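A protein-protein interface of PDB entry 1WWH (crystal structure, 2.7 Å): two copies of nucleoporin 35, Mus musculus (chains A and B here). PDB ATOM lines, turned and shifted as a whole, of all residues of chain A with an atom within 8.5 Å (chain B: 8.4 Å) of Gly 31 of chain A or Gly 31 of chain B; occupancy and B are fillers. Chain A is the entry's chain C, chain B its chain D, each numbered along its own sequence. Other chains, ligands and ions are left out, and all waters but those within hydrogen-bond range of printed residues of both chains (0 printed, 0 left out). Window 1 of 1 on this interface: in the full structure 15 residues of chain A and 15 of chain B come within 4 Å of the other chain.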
ATOM      1  N   THR A  28      29.934  29.169 -10.391  1.00  0.00           N
ATOM      2  CA  THR A  28      29.767  27.835  -9.853  1.00  0.00           C
ATOM      3  C   THR A  28      28.487  27.302 -10.499  1.00  0.00           C
ATOM      4  O   THR A  28      27.451  27.942 -10.447  1.00  0.00           O
ATOM      5  CB  THR A  28      29.725  27.829  -8.302  1.00  0.00           C
ATOM      6  OG1 THR A  28      28.612  27.060  -7.846  1.00  0.00           O
ATOM      7  CG2 THR A  28      29.647  29.211  -7.771  1.00  0.00           C
ATOM      8  N   VAL A  29      28.594  26.160 -11.167  1.00  0.00           N
ATOM      9  CA  VAL A  29      27.479  25.544 -11.871  1.00  0.00           C
ATOM     10  C   VAL A  29      26.903  24.424 -11.014  1.00  0.00           C
ATOM     11  O   VAL A  29      27.660  23.716 -10.356  1.00  0.00           O
ATOM     12  CB  VAL A  29      27.979  24.973 -13.210  1.00  0.00           C
ATOM     13  CG1 VAL A  29      26.885  24.184 -13.901  1.00  0.00           C
ATOM     14  CG2 VAL A  29      28.452  26.097 -14.087  1.00  0.00           C
ATOM     15  N   PHE A  30      25.583  24.241 -11.017  1.00  0.00           N
ATOM     16  CA  PHE A  30      24.992  23.189 -10.185  1.00  0.00           C
ATOM     17  C   PHE A  30      23.681  22.599 -10.678  1.00  0.00           C
ATOM     18  O   PHE A  30      23.076  23.101 -11.626  1.00  0.00           O
ATOM     19  CB  PHE A  30      24.786  23.713  -8.766  1.00  0.00           C
ATOM     20  CG  PHE A  30      23.822  24.849  -8.684  1.00  0.00           C
ATOM     21  CD1 PHE A  30      22.457  24.611  -8.492  1.00  0.00           C
ATOM     22  CD2 PHE A  30      24.263  26.164  -8.830  1.00  0.00           C
ATOM     23  CE1 PHE A  30      21.547  25.680  -8.451  1.00  0.00           C
ATOM     24  CE2 PHE A  30      23.360  27.238  -8.793  1.00  0.00           C
ATOM     25  CZ  PHE A  30      22.003  26.993  -8.601  1.00  0.00           C
ATOM     26  N   GLY A  31      23.259  21.518 -10.026  1.00  0.00           N
ATOM     27  CA  GLY A  31      22.013  20.862 -10.376  1.00  0.00           C
ATOM     28  C   GLY A  31      22.089  19.594 -11.207  1.00  0.00           C
ATOM     29  O   GLY A  31      21.086  19.128 -11.730  1.00  0.00           O
ATOM     30  N   PHE A  32      23.271  19.011 -11.312  1.00  0.00           N
ATOM     31  CA  PHE A  32      23.455  17.804 -12.118  1.00  0.00           C
ATOM     32  C   PHE A  32      24.020  16.649 -11.291  1.00  0.00           C
ATOM     33  O   PHE A  32      24.825  16.859 -10.365  1.00  0.00           O
ATOM     34  CB  PHE A  32      24.448  18.095 -13.243  1.00  0.00           C
ATOM     35  CG  PHE A  32      25.735  18.636 -12.739  1.00  0.00           C
ATOM     36  CD1 PHE A  32      25.889  19.996 -12.542  1.00  0.00           C
ATOM     37  CD2 PHE A  32      26.750  17.773 -12.338  1.00  0.00           C
ATOM     38  CE1 PHE A  32      27.033  20.486 -11.950  1.00  0.00           C
ATOM     39  CE2 PHE A  32      27.901  18.248 -11.739  1.00  0.00           C
ATOM     40  CZ  PHE A  32      28.047  19.603 -11.542  1.00  0.00           C
ATOM     41  N   PRO A  33      23.626  15.413 -11.638  1.00  0.00           N
ATOM     42  CA  PRO A  33      24.079  14.195 -10.954  1.00  0.00           C
ATOM     43  C   PRO A  33      25.569  13.910 -11.237  1.00  0.00           C
ATOM     44  O   PRO A  33      26.087  14.296 -12.292  1.00  0.00           O
ATOM     45  CB  PRO A  33      23.146  13.133 -11.518  1.00  0.00           C
ATOM     46  CG  PRO A  33      22.828  13.658 -12.901  1.00  0.00           C
ATOM     47  CD  PRO A  33      22.605  15.105 -12.659  1.00  0.00           C
ATOM     48  N   GLN A  34      26.251  13.248 -10.300  1.00  0.00           N
ATOM     49  CA  GLN A  34      27.681  12.928 -10.446  1.00  0.00           C
ATOM     50  C   GLN A  34      28.051  12.429 -11.839  1.00  0.00           C
ATOM     51  O   GLN A  34      29.056  12.839 -12.401  1.00  0.00           O
ATOM     52  CB  GLN A  34      28.105  11.861  -9.424  1.00  0.00           C
ATOM     53  CG  GLN A  34      28.078  12.276  -7.936  1.00  0.00           C
ATOM     54  CD  GLN A  34      29.258  13.171  -7.527  1.00  0.00           C
ATOM     55  OE1 GLN A  34      29.480  13.431  -6.330  1.00  0.00           O
ATOM     56  NE2 GLN A  34      30.014  13.652  -8.523  1.00  0.00           N
ATOM     57  N   SER A  36      26.925  13.166 -14.719  1.00  0.00           N
ATOM     58  CA  SER A  36      26.827  14.118 -15.826  1.00  0.00           C
ATOM     59  C   SER A  36      27.858  15.203 -15.694  1.00  0.00           C
ATOM     60  O   SER A  36      27.916  16.098 -16.537  1.00  0.00           O
ATOM     61  CB  SER A  36      25.451  14.778 -15.867  1.00  0.00           C
ATOM     62  OG  SER A  36      24.453  13.845 -16.201  1.00  0.00           O
ATOM     63  N   ILE A  40      28.596  18.137 -18.462  1.00  0.00           N
ATOM     64  CA  ILE A  40      28.212  19.516 -18.165  1.00  0.00           C
ATOM     65  C   ILE A  40      29.423  20.430 -18.313  1.00  0.00           C
ATOM     66  O   ILE A  40      29.323  21.542 -18.844  1.00  0.00           O
ATOM     67  CB  ILE A  40      27.620  19.649 -16.711  1.00  0.00           C
ATOM     68  CG1 ILE A  40      26.251  18.971 -16.635  1.00  0.00           C
ATOM     69  CG2 ILE A  40      27.486  21.115 -16.321  1.00  0.00           C
ATOM     70  CD1 ILE A  40      25.213  19.540 -17.628  1.00  0.00           C
ATOM     71  N   GLY A  59      28.813  17.465  -3.214  1.00  0.00           N
ATOM     72  CA  GLY A  59      27.725  18.186  -3.864  1.00  0.00           C
ATOM     73  C   GLY A  59      27.533  18.118  -5.372  1.00  0.00           C
ATOM     74  O   GLY A  59      28.449  17.801  -6.118  1.00  0.00           O
ATOM     75  N   ASN A  60      26.316  18.442  -5.805  1.00  0.00           N
ATOM     76  CA  ASN A  60      25.924  18.450  -7.211  1.00  0.00           C
ATOM     77  C   ASN A  60      26.361  19.742  -7.881  1.00  0.00           C
ATOM     78  O   ASN A  60      25.602  20.354  -8.631  1.00  0.00           O
ATOM     79  CB  ASN A  60      24.408  18.301  -7.332  1.00  0.00           C
ATOM     80  CG  ASN A  60      23.644  19.429  -6.627  1.00  0.00           C
ATOM     81  OD1 ASN A  60      24.144  20.044  -5.679  1.00  0.00           O
ATOM     82  ND2 ASN A  60      22.420  19.691  -7.079  1.00  0.00           N
ATOM     83  N   TRP A  61      27.594  20.160  -7.617  1.00  0.00           N
ATOM     84  CA  TRP A  61      28.104  21.387  -8.224  1.00  0.00           C
ATOM     85  C   TRP A  61      29.613  21.397  -8.461  1.00  0.00           C
ATOM     86  O   TRP A  61      30.356  20.631  -7.855  1.00  0.00           O
ATOM     87  CB  TRP A  61      27.743  22.587  -7.350  1.00  0.00           C
ATOM     88  CG  TRP A  61      28.418  22.586  -6.025  1.00  0.00           C
ATOM     89  CD1 TRP A  61      29.665  23.048  -5.745  1.00  0.00           C
ATOM     90  CD2 TRP A  61      27.886  22.087  -4.799  1.00  0.00           C
ATOM     91  NE1 TRP A  61      29.946  22.872  -4.416  1.00  0.00           N
ATOM     92  CE2 TRP A  61      28.870  22.284  -3.809  1.00  0.00           C
ATOM     93  CE3 TRP A  61      26.666  21.492  -4.436  1.00  0.00           C
ATOM     94  CZ2 TRP A  61      28.682  21.908  -2.473  1.00  0.00           C
ATOM     95  CZ3 TRP A  61      26.472  21.113  -3.097  1.00  0.00           C
ATOM     96  CH2 TRP A  61      27.478  21.325  -2.134  1.00  0.00           C
ATOM     97  N   MET A  62      30.041  22.275  -9.357  1.00  0.00           N
ATOM     98  CA  MET A  62      31.442  22.448  -9.670  1.00  0.00           C
ATOM     99  C   MET A  62      31.665  23.958  -9.755  1.00  0.00           C
ATOM    100  O   MET A  62      30.714  24.724  -9.955  1.00  0.00           O
ATOM    101  CB  MET A  62      31.810  21.754 -11.008  1.00  0.00           C
ATOM    102  CG  MET A  62      31.160  22.300 -12.295  1.00  0.00           C
ATOM    103  SD  MET A  62      31.661  21.452 -13.865  1.00  0.00           S
ATOM    104  CE  MET A  62      30.327  20.450 -14.185  1.00  0.00           C
ATOM    105  N   SER A  86      17.717  16.109 -19.774  1.00  0.00           N
ATOM    106  CA  SER A  86      16.729  16.502 -18.803  1.00  0.00           C
ATOM    107  C   SER A  86      17.440  17.064 -17.577  1.00  0.00           C
ATOM    108  O   SER A  86      17.220  16.609 -16.438  1.00  0.00           O
ATOM    109  CB  SER A  86      16.051  15.217 -18.445  1.00  0.00           C
ATOM    110  OG  SER A  86      17.102  14.235 -18.442  1.00  0.00           O
ATOM    111  N   ILE A  87      18.311  18.033 -17.815  1.00  0.00           N
ATOM    112  CA  ILE A  87      19.062  18.628 -16.737  1.00  0.00           C
ATOM    113  C   ILE A  87      18.919  20.154 -16.735  1.00  0.00           C
ATOM    114  O   ILE A  87      19.489  20.829 -17.588  1.00  0.00           O
ATOM    115  CB  ILE A  87      20.574  18.256 -16.846  1.00  0.00           C
ATOM    116  CG1 ILE A  87      20.733  16.750 -17.017  1.00  0.00           C
ATOM    117  CG2 ILE A  87      21.318  18.666 -15.586  1.00  0.00           C
ATOM    118  CD1 ILE A  87      22.170  16.305 -17.285  1.00  0.00           C
ATOM    119  N   MET A  88      18.140  20.693 -15.798  1.00  0.00           N
ATOM    120  CA  MET A  88      18.019  22.144 -15.678  1.00  0.00           C
ATOM    121  C   MET A  88      19.293  22.488 -14.888  1.00  0.00           C
ATOM    122  O   MET A  88      19.683  21.783 -13.947  1.00  0.00           O
ATOM    123  CB  MET A  88      16.742  22.527 -14.913  1.00  0.00           C
ATOM    124  CG  MET A  88      16.372  24.002 -14.953  1.00  0.00           C
ATOM    125  SD  MET A  88      14.669  24.233 -14.520  1.00  0.00           S
ATOM    126  CE  MET A  88      13.892  23.564 -15.894  1.00  0.00           C
ATOM    127  N   ILE A  89      19.963  23.556 -15.289  1.00  0.00           N
ATOM    128  CA  ILE A  89      21.210  23.913 -14.643  1.00  0.00           C
ATOM    129  C   ILE A  89      21.150  25.268 -13.981  1.00  0.00           C
ATOM    130  O   ILE A  89      20.542  26.208 -14.497  1.00  0.00           O
ATOM    131  CB  ILE A  89      22.369  23.897 -15.681  1.00  0.00           C
ATOM    132  CG1 ILE A  89      22.648  22.466 -16.126  1.00  0.00           C
ATOM    133  CG2 ILE A  89      23.637  24.492 -15.083  1.00  0.00           C
ATOM    134  CD1 ILE A  89      23.285  21.594 -15.039  1.00  0.00           C
ATOM    135  N   GLY A  90      21.777  25.363 -12.820  1.00  0.00           N
ATOM    136  CA  GLY A  90      21.809  26.626 -12.129  1.00  0.00           C
ATOM    137  C   GLY A  90      23.222  27.137 -12.246  1.00  0.00           C
ATOM    138  O   GLY A  90      24.158  26.345 -12.213  1.00  0.00           O
ATOM    139  N   VAL A  91      23.383  28.446 -12.402  1.00  0.00           N
ATOM    140  CA  VAL A  91      24.705  29.060 -12.515  1.00  0.00           C
ATOM    141  C   VAL A  91      24.666  30.346 -11.702  1.00  0.00           C
ATOM    142  O   VAL A  91      23.755  31.153 -11.851  1.00  0.00           O
ATOM    143  CB  VAL A  91      25.037  29.425 -13.978  1.00  0.00           C
ATOM    144  CG1 VAL A  91      26.507  29.666 -14.120  1.00  0.00           C
ATOM    145  CG2 VAL A  91      24.575  28.331 -14.928  1.00  0.00           C
ATOM    146  N   THR B  28       9.466  27.104 -10.282  1.00  0.00           N
ATOM    147  CA  THR B  28       9.953  25.770 -10.636  1.00  0.00           C
ATOM    148  C   THR B  28      11.268  25.505  -9.891  1.00  0.00           C
ATOM    149  O   THR B  28      12.209  26.289  -9.949  1.00  0.00           O
ATOM    150  CB  THR B  28      10.118  25.532 -12.189  1.00  0.00           C
ATOM    151  OG1 THR B  28      11.405  25.964 -12.611  1.00  0.00           O
ATOM    152  CG2 THR B  28       9.071  26.287 -12.981  1.00  0.00           C
ATOM    153  N   VAL B  29      11.299  24.401  -9.162  1.00  0.00           N
ATOM    154  CA  VAL B  29      12.453  24.013  -8.374  1.00  0.00           C
ATOM    155  C   VAL B  29      13.242  22.974  -9.120  1.00  0.00           C
ATOM    156  O   VAL B  29      12.665  22.034  -9.647  1.00  0.00           O
ATOM    157  CB  VAL B  29      12.006  23.407  -7.049  1.00  0.00           C
ATOM    158  CG1 VAL B  29      13.204  23.124  -6.185  1.00  0.00           C
ATOM    159  CG2 VAL B  29      11.045  24.350  -6.352  1.00  0.00           C
ATOM    160  N   PHE B  30      14.560  23.110  -9.165  1.00  0.00           N
ATOM    161  CA  PHE B  30      15.344  22.133  -9.900  1.00  0.00           C
ATOM    162  C   PHE B  30      16.697  21.789  -9.313  1.00  0.00           C
ATOM    163  O   PHE B  30      17.180  22.446  -8.387  1.00  0.00           O
ATOM    164  CB  PHE B  30      15.532  22.612 -11.342  1.00  0.00           C
ATOM    165  CG  PHE B  30      16.280  23.903 -11.459  1.00  0.00           C
ATOM    166  CD1 PHE B  30      17.672  23.906 -11.609  1.00  0.00           C
ATOM    167  CD2 PHE B  30      15.600  25.126 -11.399  1.00  0.00           C
ATOM    168  CE1 PHE B  30      18.386  25.112 -11.699  1.00  0.00           C
ATOM    169  CE2 PHE B  30      16.299  26.346 -11.487  1.00  0.00           C
ATOM    170  CZ  PHE B  30      17.698  26.338 -11.637  1.00  0.00           C
ATOM    171  N   GLY B  31      17.286  20.722  -9.851  1.00  0.00           N
ATOM    172  CA  GLY B  31      18.614  20.307  -9.445  1.00  0.00           C
ATOM    173  C   GLY B  31      18.755  19.182  -8.457  1.00  0.00           C
ATOM    174  O   GLY B  31      19.790  19.045  -7.818  1.00  0.00           O
ATOM    175  N   PHE B  32      17.740  18.350  -8.335  1.00  0.00           N
ATOM    176  CA  PHE B  32      17.810  17.247  -7.382  1.00  0.00           C
ATOM    177  C   PHE B  32      17.538  15.917  -8.092  1.00  0.00           C
ATOM    178  O   PHE B  32      16.817  15.873  -9.099  1.00  0.00           O
ATOM    179  CB  PHE B  32      16.761  17.466  -6.298  1.00  0.00           C
ATOM    180  CG  PHE B  32      15.413  17.747  -6.854  1.00  0.00           C
ATOM    181  CD1 PHE B  32      15.019  19.050  -7.115  1.00  0.00           C
ATOM    182  CD2 PHE B  32      14.578  16.705  -7.226  1.00  0.00           C
ATOM    183  CE1 PHE B  32      13.821  19.306  -7.738  1.00  0.00           C
ATOM    184  CE2 PHE B  32      13.372  16.947  -7.856  1.00  0.00           C
ATOM    185  CZ  PHE B  32      12.988  18.240  -8.115  1.00  0.00           C
ATOM    186  N   PRO B  33      18.107  14.818  -7.575  1.00  0.00           N
ATOM    187  CA  PRO B  33      17.908  13.494  -8.167  1.00  0.00           C
ATOM    188  C   PRO B  33      16.520  13.012  -7.767  1.00  0.00           C
ATOM    189  O   PRO B  33      15.996  13.439  -6.745  1.00  0.00           O
ATOM    190  CB  PRO B  33      18.995  12.668  -7.519  1.00  0.00           C
ATOM    191  CG  PRO B  33      19.019  13.244  -6.137  1.00  0.00           C
ATOM    192  CD  PRO B  33      18.970  14.738  -6.385  1.00  0.00           C
ATOM    193  N   GLN B  34      15.940  12.124  -8.573  1.00  0.00           N
ATOM    194  CA  GLN B  34      14.606  11.583  -8.318  1.00  0.00           C
ATOM    195  C   GLN B  34      14.470  11.153  -6.867  1.00  0.00           C
ATOM    196  O   GLN B  34      13.480  11.448  -6.204  1.00  0.00           O
ATOM    197  CB  GLN B  34      14.334  10.383  -9.234  1.00  0.00           C
ATOM    198  CG  GLN B  34      14.083  10.728 -10.708  1.00  0.00           C
ATOM    199  CD  GLN B  34      12.750  11.461 -10.944  1.00  0.00           C
ATOM    200  OE1 GLN B  34      12.368  11.745 -12.097  1.00  0.00           O
ATOM    201  NE2 GLN B  34      12.036  11.771  -9.850  1.00  0.00           N
ATOM    202  N   SER B  36      15.634  12.239  -4.200  1.00  0.00           N
ATOM    203  CA  SER B  36      15.329  13.304  -3.269  1.00  0.00           C
ATOM    204  C   SER B  36      14.106  14.151  -3.592  1.00  0.00           C
ATOM    205  O   SER B  36      13.838  15.112  -2.878  1.00  0.00           O
ATOM    206  CB  SER B  36      16.551  14.209  -3.104  1.00  0.00           C
ATOM    207  OG  SER B  36      17.486  13.644  -2.194  1.00  0.00           O
ATOM    208  N   ILE B  40      12.455  17.250  -1.228  1.00  0.00           N
ATOM    209  CA  ILE B  40      12.514  18.642  -1.650  1.00  0.00           C
ATOM    210  C   ILE B  40      11.127  19.269  -1.611  1.00  0.00           C
ATOM    211  O   ILE B  40      10.977  20.418  -1.179  1.00  0.00           O
ATOM    212  CB  ILE B  40      13.157  18.773  -3.064  1.00  0.00           C
ATOM    213  CG1 ILE B  40      14.612  18.296  -2.998  1.00  0.00           C
ATOM    214  CG2 ILE B  40      13.103  20.213  -3.568  1.00  0.00           C
ATOM    215  CD1 ILE B  40      15.444  18.986  -1.936  1.00  0.00           C
ATOM    216  N   GLY B  59      12.860  15.125 -16.369  1.00  0.00           N
ATOM    217  CA  GLY B  59      13.786  16.140 -15.883  1.00  0.00           C
ATOM    218  C   GLY B  59      14.063  16.137 -14.386  1.00  0.00           C
ATOM    219  O   GLY B  59      13.465  15.367 -13.628  1.00  0.00           O
ATOM    220  N   ASN B  60      14.982  17.001 -13.964  1.00  0.00           N
ATOM    221  CA  ASN B  60      15.341  17.133 -12.557  1.00  0.00           C
ATOM    222  C   ASN B  60      14.700  18.421 -12.017  1.00  0.00           C
ATOM    223  O   ASN B  60      15.380  19.270 -11.429  1.00  0.00           O
ATOM    224  CB  ASN B  60      16.865  17.210 -12.403  1.00  0.00           C
ATOM    225  CG  ASN B  60      17.465  18.442 -13.076  1.00  0.00           C
ATOM    226  OD1 ASN B  60      16.982  18.888 -14.111  1.00  0.00           O
ATOM    227  ND2 ASN B  60      18.527  18.983 -12.498  1.00  0.00           N
ATOM    228  N   TRP B  61      13.391  18.560 -12.218  1.00  0.00           N
ATOM    229  CA  TRP B  61      12.675  19.748 -11.779  1.00  0.00           C
ATOM    230  C   TRP B  61      11.196  19.492 -11.585  1.00  0.00           C
ATOM    231  O   TRP B  61      10.623  18.595 -12.211  1.00  0.00           O
ATOM    232  CB  TRP B  61      12.832  20.853 -12.805  1.00  0.00           C
ATOM    233  CG  TRP B  61      12.184  20.540 -14.106  1.00  0.00           C
ATOM    234  CD1 TRP B  61      10.860  20.634 -14.406  1.00  0.00           C
ATOM    235  CD2 TRP B  61      12.839  20.121 -15.301  1.00  0.00           C
ATOM    236  NE1 TRP B  61      10.645  20.307 -15.724  1.00  0.00           N
ATOM    237  CE2 TRP B  61      11.846  19.986 -16.299  1.00  0.00           C
ATOM    238  CE3 TRP B  61      14.176  19.842 -15.633  1.00  0.00           C
ATOM    239  CZ2 TRP B  61      12.141  19.587 -17.607  1.00  0.00           C
ATOM    240  CZ3 TRP B  61      14.469  19.445 -16.934  1.00  0.00           C
ATOM    241  CH2 TRP B  61      13.457  19.323 -17.902  1.00  0.00           C
ATOM    242  N   MET B  62      10.582  20.299 -10.724  1.00  0.00           N
ATOM    243  CA  MET B  62       9.160  20.195 -10.428  1.00  0.00           C
ATOM    244  C   MET B  62       8.590  21.614 -10.477  1.00  0.00           C
ATOM    245  O   MET B  62       9.326  22.598 -10.359  1.00  0.00           O
ATOM    246  CB  MET B  62       8.930  19.541  -9.034  1.00  0.00           C
ATOM    247  CG  MET B  62       9.159  20.451  -7.804  1.00  0.00           C
ATOM    248  SD  MET B  62       9.300  19.600  -6.203  1.00  0.00           S
ATOM    249  CE  MET B  62       7.931  18.632  -6.247  1.00  0.00           C
ATOM    250  N   SER B  86      23.988  18.184   0.865  1.00  0.00           N
ATOM    251  CA  SER B  86      24.757  18.786  -0.207  1.00  0.00           C
ATOM    252  C   SER B  86      23.990  18.726  -1.549  1.00  0.00           C
ATOM    253  O   SER B  86      24.491  18.188  -2.535  1.00  0.00           O
ATOM    254  CB  SER B  86      26.082  18.056  -0.376  1.00  0.00           C
ATOM    255  OG  SER B  86      26.876  18.156   0.785  1.00  0.00           O
ATOM    256  N   ILE B  87      22.761  19.232  -1.573  1.00  0.00           N
ATOM    257  CA  ILE B  87      21.984  19.299  -2.807  1.00  0.00           C
ATOM    258  C   ILE B  87      21.716  20.789  -3.013  1.00  0.00           C
ATOM    259  O   ILE B  87      20.877  21.353  -2.323  1.00  0.00           O
ATOM    260  CB  ILE B  87      20.637  18.592  -2.686  1.00  0.00           C
ATOM    261  CG1 ILE B  87      20.847  17.113  -2.399  1.00  0.00           C
ATOM    262  CG2 ILE B  87      19.878  18.690  -3.981  1.00  0.00           C
ATOM    263  CD1 ILE B  87      19.529  16.311  -2.326  1.00  0.00           C
ATOM    264  N   MET B  88      22.454  21.432  -3.921  1.00  0.00           N
ATOM    265  CA  MET B  88      22.277  22.863  -4.211  1.00  0.00           C
ATOM    266  C   MET B  88      21.074  22.941  -5.158  1.00  0.00           C
ATOM    267  O   MET B  88      21.074  22.377  -6.258  1.00  0.00           O
ATOM    268  CB  MET B  88      23.546  23.454  -4.851  1.00  0.00           C
ATOM    269  CG  MET B  88      23.547  24.964  -4.974  1.00  0.00           C
ATOM    270  SD  MET B  88      25.065  25.704  -5.644  1.00  0.00           S
ATOM    271  CE  MET B  88      26.179  25.344  -4.366  1.00  0.00           C
ATOM    272  N   ILE B  89      20.040  23.635  -4.700  1.00  0.00           N
ATOM    273  CA  ILE B  89      18.789  23.748  -5.436  1.00  0.00           C
ATOM    274  C   ILE B  89      18.655  25.026  -6.221  1.00  0.00           C
ATOM    275  O   ILE B  89      19.146  26.051  -5.803  1.00  0.00           O
ATOM    276  CB  ILE B  89      17.595  23.654  -4.458  1.00  0.00           C
ATOM    277  CG1 ILE B  89      17.572  22.264  -3.814  1.00  0.00           C
ATOM    278  CG2 ILE B  89      16.286  23.915  -5.196  1.00  0.00           C
ATOM    279  CD1 ILE B  89      17.190  21.153  -4.793  1.00  0.00           C
ATOM    280  N   GLY B  90      17.980  24.962  -7.359  1.00  0.00           N
ATOM    281  CA  GLY B  90      17.776  26.158  -8.148  1.00  0.00           C
ATOM    282  C   GLY B  90      16.304  26.504  -8.118  1.00  0.00           C
ATOM    283  O   GLY B  90      15.467  25.598  -8.022  1.00  0.00           O
ATOM    284  N   VAL B  91      15.960  27.787  -8.175  1.00  0.00           N
ATOM    285  CA  VAL B  91      14.546  28.148  -8.166  1.00  0.00           C
ATOM    286  C   VAL B  91      14.309  29.332  -9.079  1.00  0.00           C
ATOM    287  O   VAL B  91      14.929  30.374  -8.897  1.00  0.00           O
ATOM    288  CB  VAL B  91      14.060  28.553  -6.760  1.00  0.00           C
ATOM    289  CG1 VAL B  91      12.536  28.701  -6.785  1.00  0.00           C
ATOM    290  CG2 VAL B  91      14.521  27.531  -5.711  1.00  0.00           C
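O of Gly 31 of chain A is in hydrogen-bond range of ND2 of Asn 60 of chain B (2.7 Å). ND2 of Asn 60 of chain A lies within hydrogen-bond range of O of Gly 31 of chain B, 2.8 Å away. The side-chain amide oxygen of Asn 60 of chain A lies within hydrogen-bond range of the backbone NH of Met 88 of chain B (2.8 Å). O of Ser 86 of chain A sits close to OD1 of Asn 60 of chain B. N of Met 88 of chain A sits at hydrogen-bond distance from OD1 of Asn 60 of chain B, at 2.7 Å.
The backbone NH of Phe 30 of chain A sits at hydrogen-bond distance from the backbone carbonyl oxygen of Gly 90 of chain A (2.8 Å). N of Gly 31 of chain A lies within hydrogen-bond range of O of Asn 60 of chain A (3.0 Å). The backbone NH (N) of Gly 90 of chain B is in hydrogen-bond range of the backbone carbonyl oxygen (O) of Phe 30 of chain B. The backbone NH of Gly 31 of chain B is in hydrogen-bond range of the backbone carbonyl oxygen of Asn 60 of chain B (2.9 Å).
Gly 31 of chain A touches Gly 31 of chain B (O to CA, 3.6 Å). Ser 86 of chain B touches Gly 59 of chain A (O to CA, 3.5 Å). OD1 of Asn 60 of chain A touches O of Ser 86 of chain B, at 3.7 Å. Trp 61 of chain A touches Ser 86 of chain B. CE of Met 88 of chain B touches CD2 of Trp 61 of chain A, at 3.7 Å. CZ3 of Trp 61 of chain B touches C of Ser 86 of chain A, 3.9 Å away. Ile 87 of chain A touches Asn 60 of chain B. Met 88 of chain A touches Phe 30 of chain B. Met 88 of chain A touches Trp 61 of chain B (CE to CD2, 3.6 Å). Ile 89 of chain A touches Phe 30 of chain B (C to CE1, 3.6 Å).
Gly 31 of chain A touches just these residues of chain B: Gly 31 (3.6 Å) and Asn 60 (2.7 Å). Of chain A, only Gly 31 and Asn 60 come within 4 Å of Gly 31 of chain B. Of the printed residues of chain B, Gly 90 of chain A touches Phe 30. Printed residues of chain B within 4 Å of Asn 60 of chain A: Gly 31, Ser 86, Ile 87 and Met 88. Printed residues of chain B within 4 Å of Ile 89 of chain A: Phe 30 (3.6 Å). Of the printed residues of chain A, Gly 59 of chain B touches Ser 86 (3.5 Å). The nearest residue of chain B that does not touch Gly 31 of chain A is Met 88 of chain B (4.4 Å).
Of the 19 printed residues of chain B, 10 touch a printed residue of chain A. Hydrophobic or aromatic side chains of chain B that line the printed part of chain A: Phe 30, Trp 61 and Met 88. Hydrophobic or aromatic side chains of chain A within 4 Å of the printed part of chain B: Phe 30, Trp 61 and Met 88. Among the printed residues, no Asp or Glu carboxylate lies within 4 Å of a Lys or Arg side-chain nitrogen of the other chain.
Gly 31 of chain A touches Asn 60 of chain B, and with the chains exchanged Asn 60 of chain A touches Gly 31 of chain B. Gly 59 of chain A touches Ser 86 of chain B, and with the chains exchanged Ser 86 of chain A touches Gly 59 of chain B. Asn 60 of chain A touches Met 88 of chain B, and with the chains exchanged Met 88 of chain A touches Asn 60 of chain B. Trp 61 of chain A touches Ser 86 of chain B, and with the chains exchanged Ser 86 of chain A touches Trp 61 of chain B. 19 positions are printed for both chains.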
